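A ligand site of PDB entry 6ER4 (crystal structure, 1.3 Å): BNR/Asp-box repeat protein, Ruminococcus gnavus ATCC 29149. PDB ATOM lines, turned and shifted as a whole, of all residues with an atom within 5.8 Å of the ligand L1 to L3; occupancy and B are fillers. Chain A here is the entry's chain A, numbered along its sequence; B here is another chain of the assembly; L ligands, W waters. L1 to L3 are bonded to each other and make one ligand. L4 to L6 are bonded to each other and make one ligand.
The side-chain carboxylate (OD2) of Asp 88 of chain A is in hydrogen-bond range of an oxygen (O1) of LIG L1, 2.5 Å away.
The side-chain carboxylate (OD2) of Asp 67 lies within hydrogen-bond range of an oxygen (O6) of LIG L1 (2.6 Å).
The side-chain carboxylate (OE2) of Glu 83 lies within hydrogen-bond range of an oxygen (O3) of LG3 L3 (2.6 Å).
NZ of Lys 92 of chain A lies within hydrogen-bond range of O3 of LG3 L3 (2.8 Å).
An oxygen (O1) of LG3 L3 is in salt-bridge range of the guanidinium group (NH2) of Arg 161 (2.8 Å).
The guanidinium group (NH1) of Arg 85 is in salt-bridge range of an oxygen (O1) of LG3 L3 (3.0 Å).
A nitrogen (N1) of LG3 L3 sits at hydrogen-bond distance from the side-chain hydroxyl (OH) of Tyr 167, 3.3 Å away.
O3 of LG6 L6 lies within hydrogen-bond range of NZ of Lys 92 of chain B (2.8 Å).
OD2 of Asp 88 of chain B sits at hydrogen-bond distance from O1 of LG4 L4, 2.6 Å away.
O5 of LG3 L3 sits at hydrogen-bond distance from O3 of LG4 L4 (2.7 Å).
OD1 of Asp 88 of chain A is in salt-bridge range of NH2 of Arg 85 (2.9 Å).
OD1 of Asp 67 is in salt-bridge range of NH2 of Arg 161 (3.0 Å).
The side-chain carboxylate (OD1) of Asp 67 is in salt-bridge range of the guanidinium group (NH2) of Arg 85 (3.6 Å).
OE1 of Glu 83 sits at hydrogen-bond distance from NE2 of His 71, 2.8 Å away.
The guanidinium group of Arg 161 lies within hydrogen-bond range of the side-chain hydroxyl of Tyr 167 (3.2 Å).
NE of Arg 161 lies within hydrogen-bond range of O of Gln 66, at 2.8 Å.
Ile 52 of chain A touches the ligand L1 to L3.
Tyr 73 touches the ligand L1 to L3.
Ile 52 of chain B touches the ligand L1 to L3.
Hydrophobic or aromatic side chains that line the ligand L1 to L3: Ile 52 of chain A, Tyr 73, Tyr 167 and Ile 52 of chain B.
Water W7 bridges an oxygen (O7) of LG3 L3 (2.7 Å) and an oxygen (O3) of LG4 L4 (2.9 Å).
Water W5 lies within hydrogen-bond range of NZ of Lys 92 of chain B (2.8 Å) and O8 of LG3 L3 (3.0 Å).
Water W10 bridges O2 of LG3 L3 (3.0 Å) and NH2 of Arg 161 (3.5 Å).
Water W9 lies within hydrogen-bond range of O1 of LG2 L2 (3.0 Å) and NE2 of Gln 66 (3.5 Å).
Water W8 lies within hydrogen-bond range of O4 of LG6 L6 (2.9 Å) and O5 of LG2 L2 (3.1 Å).
Water W6 lies within hydrogen-bond range of O5 of LG3 L3 (3.1 Å) and NZ of Lys 92 of chain B (3.2 Å).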
ATOM      1  N   ILE A  52      14.184  38.424 -27.681  1.00  0.00           N
ATOM      2  CA  ILE A  52      13.427  37.792 -28.781  1.00  0.00           C
ATOM      3  C   ILE A  52      12.706  38.916 -29.539  1.00  0.00           C
ATOM      4  O   ILE A  52      11.878  39.614 -28.965  1.00  0.00           O
ATOM      5  CB  ILE A  52      12.399  36.760 -28.269  1.00  0.00           C
ATOM      6  CG1 ILE A  52      13.038  35.712 -27.365  1.00  0.00           C
ATOM      7  CG2 ILE A  52      11.733  36.107 -29.456  1.00  0.00           C
ATOM      8  CD1 ILE A  52      12.005  34.995 -26.517  1.00  0.00           C
ATOM      9  N   GLN A  66      -3.105  33.126 -27.384  1.00  0.00           N
ATOM     10  CA  GLN A  66      -1.728  33.608 -27.386  1.00  0.00           C
ATOM     11  C   GLN A  66      -0.689  32.597 -27.865  1.00  0.00           C
ATOM     12  O   GLN A  66       0.452  32.979 -28.112  1.00  0.00           O
ATOM     13  CB  GLN A  66      -1.308  34.126 -25.988  1.00  0.00           C
ATOM     14  CG  GLN A  66      -1.406  33.109 -24.849  1.00  0.00           C
ATOM     15  CD  GLN A  66      -2.749  33.024 -24.160  1.00  0.00           C
ATOM     16  OE1 GLN A  66      -3.759  33.437 -24.689  1.00  0.00           O
ATOM     17  NE2 GLN A  66      -2.752  32.477 -22.970  1.00  0.00           N
ATOM     18  N   ASP A  67      -1.046  31.321 -27.963  1.00  0.00           N
ATOM     19  CA  ASP A  67      -0.142  30.302 -28.502  1.00  0.00           C
ATOM     20  C   ASP A  67      -0.478  29.907 -29.920  1.00  0.00           C
ATOM     21  O   ASP A  67       0.010  28.867 -30.379  1.00  0.00           O
ATOM     22  CB  ASP A  67      -0.090  29.058 -27.579  1.00  0.00           C
ATOM     23  CG  ASP A  67       0.391  29.344 -26.182  1.00  0.00           C
ATOM     24  OD1 ASP A  67       1.054  30.359 -25.935  1.00  0.00           O
ATOM     25  OD2 ASP A  67       0.124  28.475 -25.310  1.00  0.00           O
ATOM     26  N   HIS A  71       5.998  33.179 -36.129  1.00  0.00           N
ATOM     27  CA  HIS A  71       6.919  34.318 -36.311  1.00  0.00           C
ATOM     28  C   HIS A  71       8.311  33.884 -36.673  1.00  0.00           C
ATOM     29  O   HIS A  71       8.737  32.763 -36.373  1.00  0.00           O
ATOM     30  CB  HIS A  71       6.933  35.247 -35.080  1.00  0.00           C
ATOM     31  CG  HIS A  71       7.568  34.665 -33.852  1.00  0.00           C
ATOM     32  ND1 HIS A  71       8.498  35.359 -33.094  1.00  0.00           N
ATOM     33  CD2 HIS A  71       7.368  33.481 -33.212  1.00  0.00           C
ATOM     34  CE1 HIS A  71       8.820  34.650 -32.044  1.00  0.00           C
ATOM     35  NE2 HIS A  71       8.164  33.499 -32.092  1.00  0.00           N
ATOM     36  N   TYR A  73      12.088  35.357 -36.109  1.00  0.00           N
ATOM     37  CA  TYR A  73      12.648  36.246 -35.088  1.00  0.00           C
ATOM     38  C   TYR A  73      14.179  36.195 -35.073  1.00  0.00           C
ATOM     39  O   TYR A  73      14.783  35.256 -35.585  1.00  0.00           O
ATOM     40  CB  TYR A  73      12.103  35.932 -33.700  1.00  0.00           C
ATOM     41  CG  TYR A  73      12.519  34.621 -33.116  1.00  0.00           C
ATOM     42  CD1 TYR A  73      13.719  34.503 -32.404  1.00  0.00           C
ATOM     43  CD2 TYR A  73      11.759  33.473 -33.275  1.00  0.00           C
ATOM     44  CE1 TYR A  73      14.113  33.309 -31.841  1.00  0.00           C
ATOM     45  CE2 TYR A  73      12.157  32.281 -32.699  1.00  0.00           C
ATOM     46  CZ  TYR A  73      13.319  32.200 -32.000  1.00  0.00           C
ATOM     47  OH  TYR A  73      13.686  31.002 -31.449  1.00  0.00           O
ATOM     48  N   GLU A  83       9.039  30.219 -34.845  1.00  0.00           N
ATOM     49  CA  GLU A  83       8.098  29.323 -34.180  1.00  0.00           C
ATOM     50  C   GLU A  83       6.815  29.304 -34.986  1.00  0.00           C
ATOM     51  O   GLU A  83       6.317  30.343 -35.423  1.00  0.00           O
ATOM     52  CB  GLU A  83       7.789  29.724 -32.769  1.00  0.00           C
ATOM     53  CG  GLU A  83       8.976  29.959 -31.876  1.00  0.00           C
ATOM     54  CD  GLU A  83       8.527  30.252 -30.463  1.00  0.00           C
ATOM     55  OE1 GLU A  83       8.133  31.412 -30.167  1.00  0.00           O
ATOM     56  OE2 GLU A  83       8.527  29.304 -29.635  1.00  0.00           O
ATOM     57  N   ARG A  85       3.025  27.753 -34.357  1.00  0.00           N
ATOM     58  CA  ARG A  85       2.290  27.294 -33.165  1.00  0.00           C
ATOM     59  C   ARG A  85       0.791  27.355 -33.332  1.00  0.00           C
ATOM     60  O   ARG A  85       0.256  28.337 -33.885  1.00  0.00           O
ATOM     61  CB  ARG A  85       2.654  28.186 -31.987  1.00  0.00           C
ATOM     62  CG  ARG A  85       4.129  28.207 -31.675  1.00  0.00           C
ATOM     63  CD  ARG A  85       4.450  28.877 -30.342  1.00  0.00           C
ATOM     64  NE  ARG A  85       3.841  28.116 -29.245  1.00  0.00           N
ATOM     65  CZ  ARG A  85       3.807  28.544 -27.973  1.00  0.00           C
ATOM     66  NH1 ARG A  85       4.293  29.742 -27.640  1.00  0.00           N
ATOM     67  NH2 ARG A  85       3.247  27.795 -27.044  1.00  0.00           N
ATOM     68  N   ASP A  88       0.243  23.983 -27.923  1.00  0.00           N
ATOM     69  CA  ASP A  88       1.203  22.869 -27.910  1.00  0.00           C
ATOM     70  C   ASP A  88       0.541  21.505 -28.126  1.00  0.00           C
ATOM     71  O   ASP A  88       1.163  20.613 -28.628  1.00  0.00           O
ATOM     72  CB  ASP A  88       2.030  22.891 -26.619  1.00  0.00           C
ATOM     73  CG  ASP A  88       2.914  24.123 -26.467  1.00  0.00           C
ATOM     74  OD1 ASP A  88       3.071  24.882 -27.434  1.00  0.00           O
ATOM     75  OD2 ASP A  88       3.431  24.306 -25.364  1.00  0.00           O
ATOM     76  N   GLY A  89      -0.719  21.402 -27.745  1.00  0.00           N
ATOM     77  CA  GLY A  89      -1.500  20.187 -27.995  1.00  0.00           C
ATOM     78  C   GLY A  89      -1.740  19.890 -29.465  1.00  0.00           C
ATOM     79  O   GLY A  89      -1.973  18.741 -29.831  1.00  0.00           O
ATOM     80  N   LYS A  92       3.839  22.610 -32.126  1.00  0.00           N
ATOM     81  CA  LYS A  92       4.840  23.645 -31.819  1.00  0.00           C
ATOM     82  C   LYS A  92       6.121  23.291 -32.531  1.00  0.00           C
ATOM     83  O   LYS A  92       6.886  22.439 -32.097  1.00  0.00           O
ATOM     84  CB  LYS A  92       5.085  23.730 -30.314  1.00  0.00           C
ATOM     85  CG  LYS A  92       6.004  24.887 -29.967  1.00  0.00           C
ATOM     86  CD  LYS A  92       6.319  24.976 -28.492  1.00  0.00           C
ATOM     87  CE  LYS A  92       7.119  26.248 -28.243  1.00  0.00           C
ATOM     88  NZ  LYS A  92       7.494  26.370 -26.811  1.00  0.00           N
ATOM     89  N   THR A  94       9.645  24.565 -34.176  1.00  0.00           N
ATOM     90  CA  THR A  94      10.563  25.673 -33.938  1.00  0.00           C
ATOM     91  C   THR A  94      11.940  25.396 -34.492  1.00  0.00           C
ATOM     92  O   THR A  94      12.358  24.246 -34.653  1.00  0.00           O
ATOM     93  CB  THR A  94      10.695  25.954 -32.429  1.00  0.00           C
ATOM     94  OG1 THR A  94      11.440  24.923 -31.824  1.00  0.00           O
ATOM     95  CG2 THR A  94       9.387  26.124 -31.743  1.00  0.00           C
ATOM     96  N   ASP A  96      15.940  27.402 -33.875  1.00  0.00           N
ATOM     97  CA  ASP A  96      16.741  28.399 -33.181  1.00  0.00           C
ATOM     98  C   ASP A  96      18.194  28.110 -33.488  1.00  0.00           C
ATOM     99  O   ASP A  96      18.694  27.018 -33.182  1.00  0.00           O
ATOM    100  CB  ASP A  96      16.474  28.357 -31.682  1.00  0.00           C
ATOM    101  CG  ASP A  96      16.837  29.600 -31.043  1.00  0.00           C
ATOM    102  OD1 ASP A  96      18.030  29.720 -30.752  1.00  0.00           O
ATOM    103  OD2 ASP A  96      15.967  30.505 -30.918  1.00  0.00           O
ATOM    104  N   ARG A 161      -0.281  39.014 -29.011  1.00  0.00           N
ATOM    105  CA  ARG A 161      -0.662  37.979 -28.047  1.00  0.00           C
ATOM    106  C   ARG A 161      -1.647  38.646 -27.090  1.00  0.00           C
ATOM    107  O   ARG A 161      -1.262  39.502 -26.292  1.00  0.00           O
ATOM    108  CB  ARG A 161       0.550  37.432 -27.320  1.00  0.00           C
ATOM    109  CG  ARG A 161       1.615  36.868 -28.278  1.00  0.00           C
ATOM    110  CD  ARG A 161       2.747  36.161 -27.536  1.00  0.00           C
ATOM    111  NE  ARG A 161       2.355  34.834 -27.121  1.00  0.00           N
ATOM    112  CZ  ARG A 161       3.099  34.046 -26.379  1.00  0.00           C
ATOM    113  NH1 ARG A 161       4.174  34.515 -25.795  1.00  0.00           N
ATOM    114  NH2 ARG A 161       2.714  32.797 -26.146  1.00  0.00           N
ATOM    115  N   TYR A 167       7.437  39.935 -28.046  1.00  0.00           N
ATOM    116  CA  TYR A 167       8.685  39.693 -28.806  1.00  0.00           C
ATOM    117  C   TYR A 167       9.108  40.950 -29.594  1.00  0.00           C
ATOM    118  O   TYR A 167       9.269  40.937 -30.812  1.00  0.00           O
ATOM    119  CB  TYR A 167       8.573  38.499 -29.739  1.00  0.00           C
ATOM    120  CG  TYR A 167       8.077  37.207 -29.093  1.00  0.00           C
ATOM    121  CD1 TYR A 167       8.522  36.791 -27.849  1.00  0.00           C
ATOM    122  CD2 TYR A 167       7.170  36.407 -29.740  1.00  0.00           C
ATOM    123  CE1 TYR A 167       8.089  35.577 -27.294  1.00  0.00           C
ATOM    124  CE2 TYR A 167       6.728  35.206 -29.213  1.00  0.00           C
ATOM    125  CZ  TYR A 167       7.168  34.796 -27.975  1.00  0.00           C
ATOM    126  OH  TYR A 167       6.790  33.594 -27.444  1.00  0.00           O
ATOM    127  N   ALA B  51       2.501  16.795 -17.711  1.00  0.00           N
ATOM    128  CA  ALA B  51       2.538  17.400 -19.046  1.00  0.00           C
ATOM    129  C   ALA B  51       3.785  17.043 -19.859  1.00  0.00           C
ATOM    130  O   ALA B  51       3.704  16.766 -21.051  1.00  0.00           O
ATOM    131  CB  ALA B  51       2.416  18.904 -18.930  1.00  0.00           C
ATOM    132  N   ILE B  52       4.959  17.098 -19.214  1.00  0.00           N
ATOM    133  CA  ILE B  52       6.234  16.855 -19.870  1.00  0.00           C
ATOM    134  C   ILE B  52       6.964  15.833 -19.029  1.00  0.00           C
ATOM    135  O   ILE B  52       7.258  16.080 -17.836  1.00  0.00           O
ATOM    136  CB  ILE B  52       7.090  18.107 -19.987  1.00  0.00           C
ATOM    137  CG1 ILE B  52       6.326  19.239 -20.698  1.00  0.00           C
ATOM    138  CG2 ILE B  52       8.412  17.813 -20.701  1.00  0.00           C
ATOM    139  CD1 ILE B  52       6.961  20.587 -20.453  1.00  0.00           C
ATOM    140  N   ASP B  88      20.464  29.369 -23.787  1.00  0.00           N
ATOM    141  CA  ASP B  88      19.963  29.754 -25.104  1.00  0.00           C
ATOM    142  C   ASP B  88      20.966  30.566 -25.937  1.00  0.00           C
ATOM    143  O   ASP B  88      20.934  30.519 -27.134  1.00  0.00           O
ATOM    144  CB  ASP B  88      18.630  30.477 -24.967  1.00  0.00           C
ATOM    145  CG  ASP B  88      17.514  29.619 -24.397  1.00  0.00           C
ATOM    146  OD1 ASP B  88      17.658  28.410 -24.270  1.00  0.00           O
ATOM    147  OD2 ASP B  88      16.466  30.218 -24.082  1.00  0.00           O
ATOM    148  N   LYS B  92      19.991  25.971 -28.361  1.00  0.00           N
ATOM    149  CA  LYS B  92      18.739  25.348 -27.944  1.00  0.00           C
ATOM    150  C   LYS B  92      18.153  24.665 -29.152  1.00  0.00           C
ATOM    151  O   LYS B  92      17.512  25.305 -29.993  1.00  0.00           O
ATOM    152  CB  LYS B  92      17.754  26.373 -27.389  1.00  0.00           C
ATOM    153  CG  LYS B  92      16.521  25.716 -26.790  1.00  0.00           C
ATOM    154  CD  LYS B  92      15.488  26.648 -26.257  1.00  0.00           C
ATOM    155  CE  LYS B  92      14.375  25.863 -25.575  1.00  0.00           C
ATOM    156  NZ  LYS B  92      13.299  26.767 -25.059  1.00  0.00           N
HETATM  157  C1  LIG L   1       3.903  24.534 -21.970  1.00  0.00           C
HETATM  158  C2  LIG L   1       3.976  25.587 -20.865  1.00  0.00           C
HETATM  159  C3  LIG L   1       3.136  26.780 -21.284  1.00  0.00           C
HETATM  160  C4  LIG L   1       1.714  26.280 -21.599  1.00  0.00           C
HETATM  161  C5  LIG L   1       0.775  27.412 -22.062  1.00  0.00           C
HETATM  162  C6  LIG L   1       2.449  24.158 -22.243  1.00  0.00           C
HETATM  163  O1  LIG L   1       2.379  23.248 -23.339  1.00  0.00           O
HETATM  164  O2  LIG L   1       4.639  23.390 -21.508  1.00  0.00           O
HETATM  165  O3  LIG L   1       5.351  25.937 -20.656  1.00  0.00           O
HETATM  166  O4  LIG L   1       3.104  27.654 -20.157  1.00  0.00           O
HETATM  167  O5  LIG L   1       1.814  25.359 -22.685  1.00  0.00           O
HETATM  168  O6  LIG L   1       1.370  28.224 -23.083  1.00  0.00           O
HETATM  169  C1  LG2 L   2       3.256  29.023 -20.489  1.00  0.00           C
HETATM  170  C2  LG2 L   2       2.852  29.832 -19.263  1.00  0.00           C
HETATM  171  C3  LG2 L   2       3.069  31.324 -19.530  1.00  0.00           C
HETATM  172  C4  LG2 L   2       4.496  31.554 -19.988  1.00  0.00           C
HETATM  173  C5  LG2 L   2       4.812  30.627 -21.168  1.00  0.00           C
HETATM  174  C6  LG2 L   2       6.246  30.812 -21.608  1.00  0.00           C
HETATM  175  O1  LG2 L   2       1.465  29.635 -18.995  1.00  0.00           O
HETATM  176  O2  LG2 L   2       2.785  32.078 -18.369  1.00  0.00           O
HETATM  177  O3  LG2 L   2       5.425  31.224 -18.944  1.00  0.00           O
HETATM  178  O4  LG2 L   2       4.601  29.242 -20.796  1.00  0.00           O
HETATM  179  O5  LG2 L   2       6.503  29.996 -22.765  1.00  0.00           O
HETATM  180  C1  LG3 L   3       5.564  31.541 -24.337  1.00  0.00           C
HETATM  181  C2  LG3 L   3       6.744  30.656 -23.998  1.00  0.00           C
HETATM  182  C3  LG3 L   3       7.047  29.564 -25.052  1.00  0.00           C
HETATM  183  C4  LG3 L   3       7.647  30.180 -26.302  1.00  0.00           C
HETATM  184  C5  LG3 L   3       8.879  31.035 -25.965  1.00  0.00           C
HETATM  185  C6  LG3 L   3       8.442  32.095 -24.945  1.00  0.00           C
HETATM  186  C7  LG3 L   3       9.534  33.036 -24.447  1.00  0.00           C
HETATM  187  C8  LG3 L   3       9.018  33.939 -23.327  1.00  0.00           C
HETATM  188  C9  LG3 L   3      10.007  35.059 -23.081  1.00  0.00           C
HETATM  189  C10 LG3 L   3      10.678  31.684 -27.469  1.00  0.00           C
HETATM  190  C11 LG3 L   3      11.040  32.183 -28.831  1.00  0.00           C
HETATM  191  N1  LG3 L   3       9.410  31.640 -27.193  1.00  0.00           N
HETATM  192  O1  LG3 L   3       4.555  31.033 -24.904  1.00  0.00           O
HETATM  193  O2  LG3 L   3       5.608  32.750 -24.018  1.00  0.00           O
HETATM  194  O3  LG3 L   3       8.028  29.080 -27.125  1.00  0.00           O
HETATM  195  O4  LG3 L   3       7.930  31.424 -23.777  1.00  0.00           O
HETATM  196  O5  LG3 L   3      10.657  32.303 -23.982  1.00  0.00           O
HETATM  197  O6  LG3 L   3       7.712  34.491 -23.631  1.00  0.00           O
HETATM  198  O7  LG3 L   3       9.694  35.732 -21.867  1.00  0.00           O
HETATM  199  O8  LG3 L   3      11.539  31.374 -26.624  1.00  0.00           O
HETATM  200  C1  LG4 L   4      14.322  32.588 -22.650  1.00  0.00           C
HETATM  201  C2  LG4 L   4      13.474  32.758 -21.413  1.00  0.00           C
HETATM  202  C3  LG4 L   4      14.069  31.926 -20.289  1.00  0.00           C
HETATM  203  C4  LG4 L   4      15.513  32.341 -20.071  1.00  0.00           C
HETATM  204  C5  LG4 L   4      16.214  31.586 -18.947  1.00  0.00           C
HETATM  205  C6  LG4 L   4      15.768  32.942 -22.341  1.00  0.00           C
HETATM  206  O1  LG4 L   4      16.633  32.723 -23.441  1.00  0.00           O
HETATM  207  O2  LG4 L   4      13.798  33.424 -23.673  1.00  0.00           O
HETATM  208  O3  LG4 L   4      12.137  32.329 -21.680  1.00  0.00           O
HETATM  209  O4  LG4 L   4      13.336  32.244 -19.110  1.00  0.00           O
HETATM  210  O5  LG4 L   4      16.217  32.099 -21.302  1.00  0.00           O
HETATM  211  O6  LG4 L   4      16.042  30.173 -19.063  1.00  0.00           O
HETATM  212  C1  LG5 L   5      12.860  31.234 -18.265  1.00  0.00           C
HETATM  213  C2  LG5 L   5      12.552  31.660 -16.850  1.00  0.00           C
HETATM  214  C3  LG5 L   5      12.105  30.482 -16.002  1.00  0.00           C
HETATM  215  C4  LG5 L   5      11.074  29.642 -16.746  1.00  0.00           C
HETATM  216  C5  LG5 L   5      11.608  29.254 -18.111  1.00  0.00           C
HETATM  217  C6  LG5 L   5      10.583  28.402 -18.856  1.00  0.00           C
HETATM  218  O1  LG5 L   5      13.677  32.344 -16.285  1.00  0.00           O
HETATM  219  O2  LG5 L   5      11.557  31.023 -14.782  1.00  0.00           O
HETATM  220  O3  LG5 L   5       9.872  30.398 -16.966  1.00  0.00           O
HETATM  221  O4  LG5 L   5      11.914  30.398 -18.906  1.00  0.00           O
HETATM  222  O5  LG5 L   5      11.169  27.985 -20.116  1.00  0.00           O
HETATM  223  C1  LG6 L   6      12.308  26.112 -19.127  1.00  0.00           C
HETATM  224  C2  LG6 L   6      11.380  26.588 -20.237  1.00  0.00           C
HETATM  225  C3  LG6 L   6      11.902  26.355 -21.634  1.00  0.00           C
HETATM  226  C4  LG6 L   6      11.882  24.877 -22.019  1.00  0.00           C
HETATM  227  C5  LG6 L   6      10.495  24.282 -21.828  1.00  0.00           C
HETATM  228  C6  LG6 L   6      10.093  24.531 -20.367  1.00  0.00           C
HETATM  229  C7  LG6 L   6       8.686  24.017 -20.001  1.00  0.00           C
HETATM  230  C8  LG6 L   6       8.281  24.489 -18.584  1.00  0.00           C
HETATM  231  C9  LG6 L   6       7.097  23.706 -18.097  1.00  0.00           C
HETATM  232  C10 LG6 L   6       9.593  22.242 -22.802  1.00  0.00           C
HETATM  233  C11 LG6 L   6       9.857  20.802 -23.192  1.00  0.00           C
HETATM  234  N1  LG6 L   6      10.545  22.865 -22.127  1.00  0.00           N
HETATM  235  O1  LG6 L   6      13.540  26.263 -19.257  1.00  0.00           O
HETATM  236  O2  LG6 L   6      11.795  25.600 -18.095  1.00  0.00           O
HETATM  237  O3  LG6 L   6      12.266  24.827 -23.400  1.00  0.00           O
HETATM  238  O4  LG6 L   6      10.084  25.973 -20.134  1.00  0.00           O
HETATM  239  O5  LG6 L   6       7.705  24.550 -20.928  1.00  0.00           O
HETATM  240  O6  LG6 L   6       9.366  24.294 -17.684  1.00  0.00           O
HETATM  241  O7  LG6 L   6       6.598  24.336 -16.909  1.00  0.00           O
HETATM  242  O8  LG6 L   6       8.535  22.809 -23.032  1.00  0.00           O
HETATM  243  O   HOH W   1       0.218  25.746 -25.627  1.00  0.00           O
HETATM  244  O   HOH W   2       0.432  27.205 -18.055  1.00  0.00           O
HETATM  245  O   HOH W   3       3.682  28.489 -24.267  1.00  0.00           O
HETATM  246  O   HOH W   4       9.705  30.062 -21.946  1.00  0.00           O
HETATM  247  O   HOH W   5      12.352  28.550 -26.952  1.00  0.00           O
HETATM  248  O   HOH W   6      11.584  29.325 -24.112  1.00  0.00           O
HETATM  249  O   HOH W   7      10.652  34.086 -19.927  1.00  0.00           O
HETATM  250  O   HOH W   8       8.114  27.714 -21.390  1.00  0.00           O
HETATM  251  O   HOH W   9      -0.363  30.754 -21.125  1.00  0.00           O
HETATM  252  O   HOH W  10       2.981  33.302 -22.722  1.00  0.00           O
HETATM  253  O   HOH W  11       6.633  28.427 -18.752  1.00  0.00           O
HETATM  254  O   HOH W  12       1.381  31.258 -23.365  1.00  0.00           O
HETATM  255  O   HOH W  13       3.595  22.038 -19.509  1.00  0.00           O
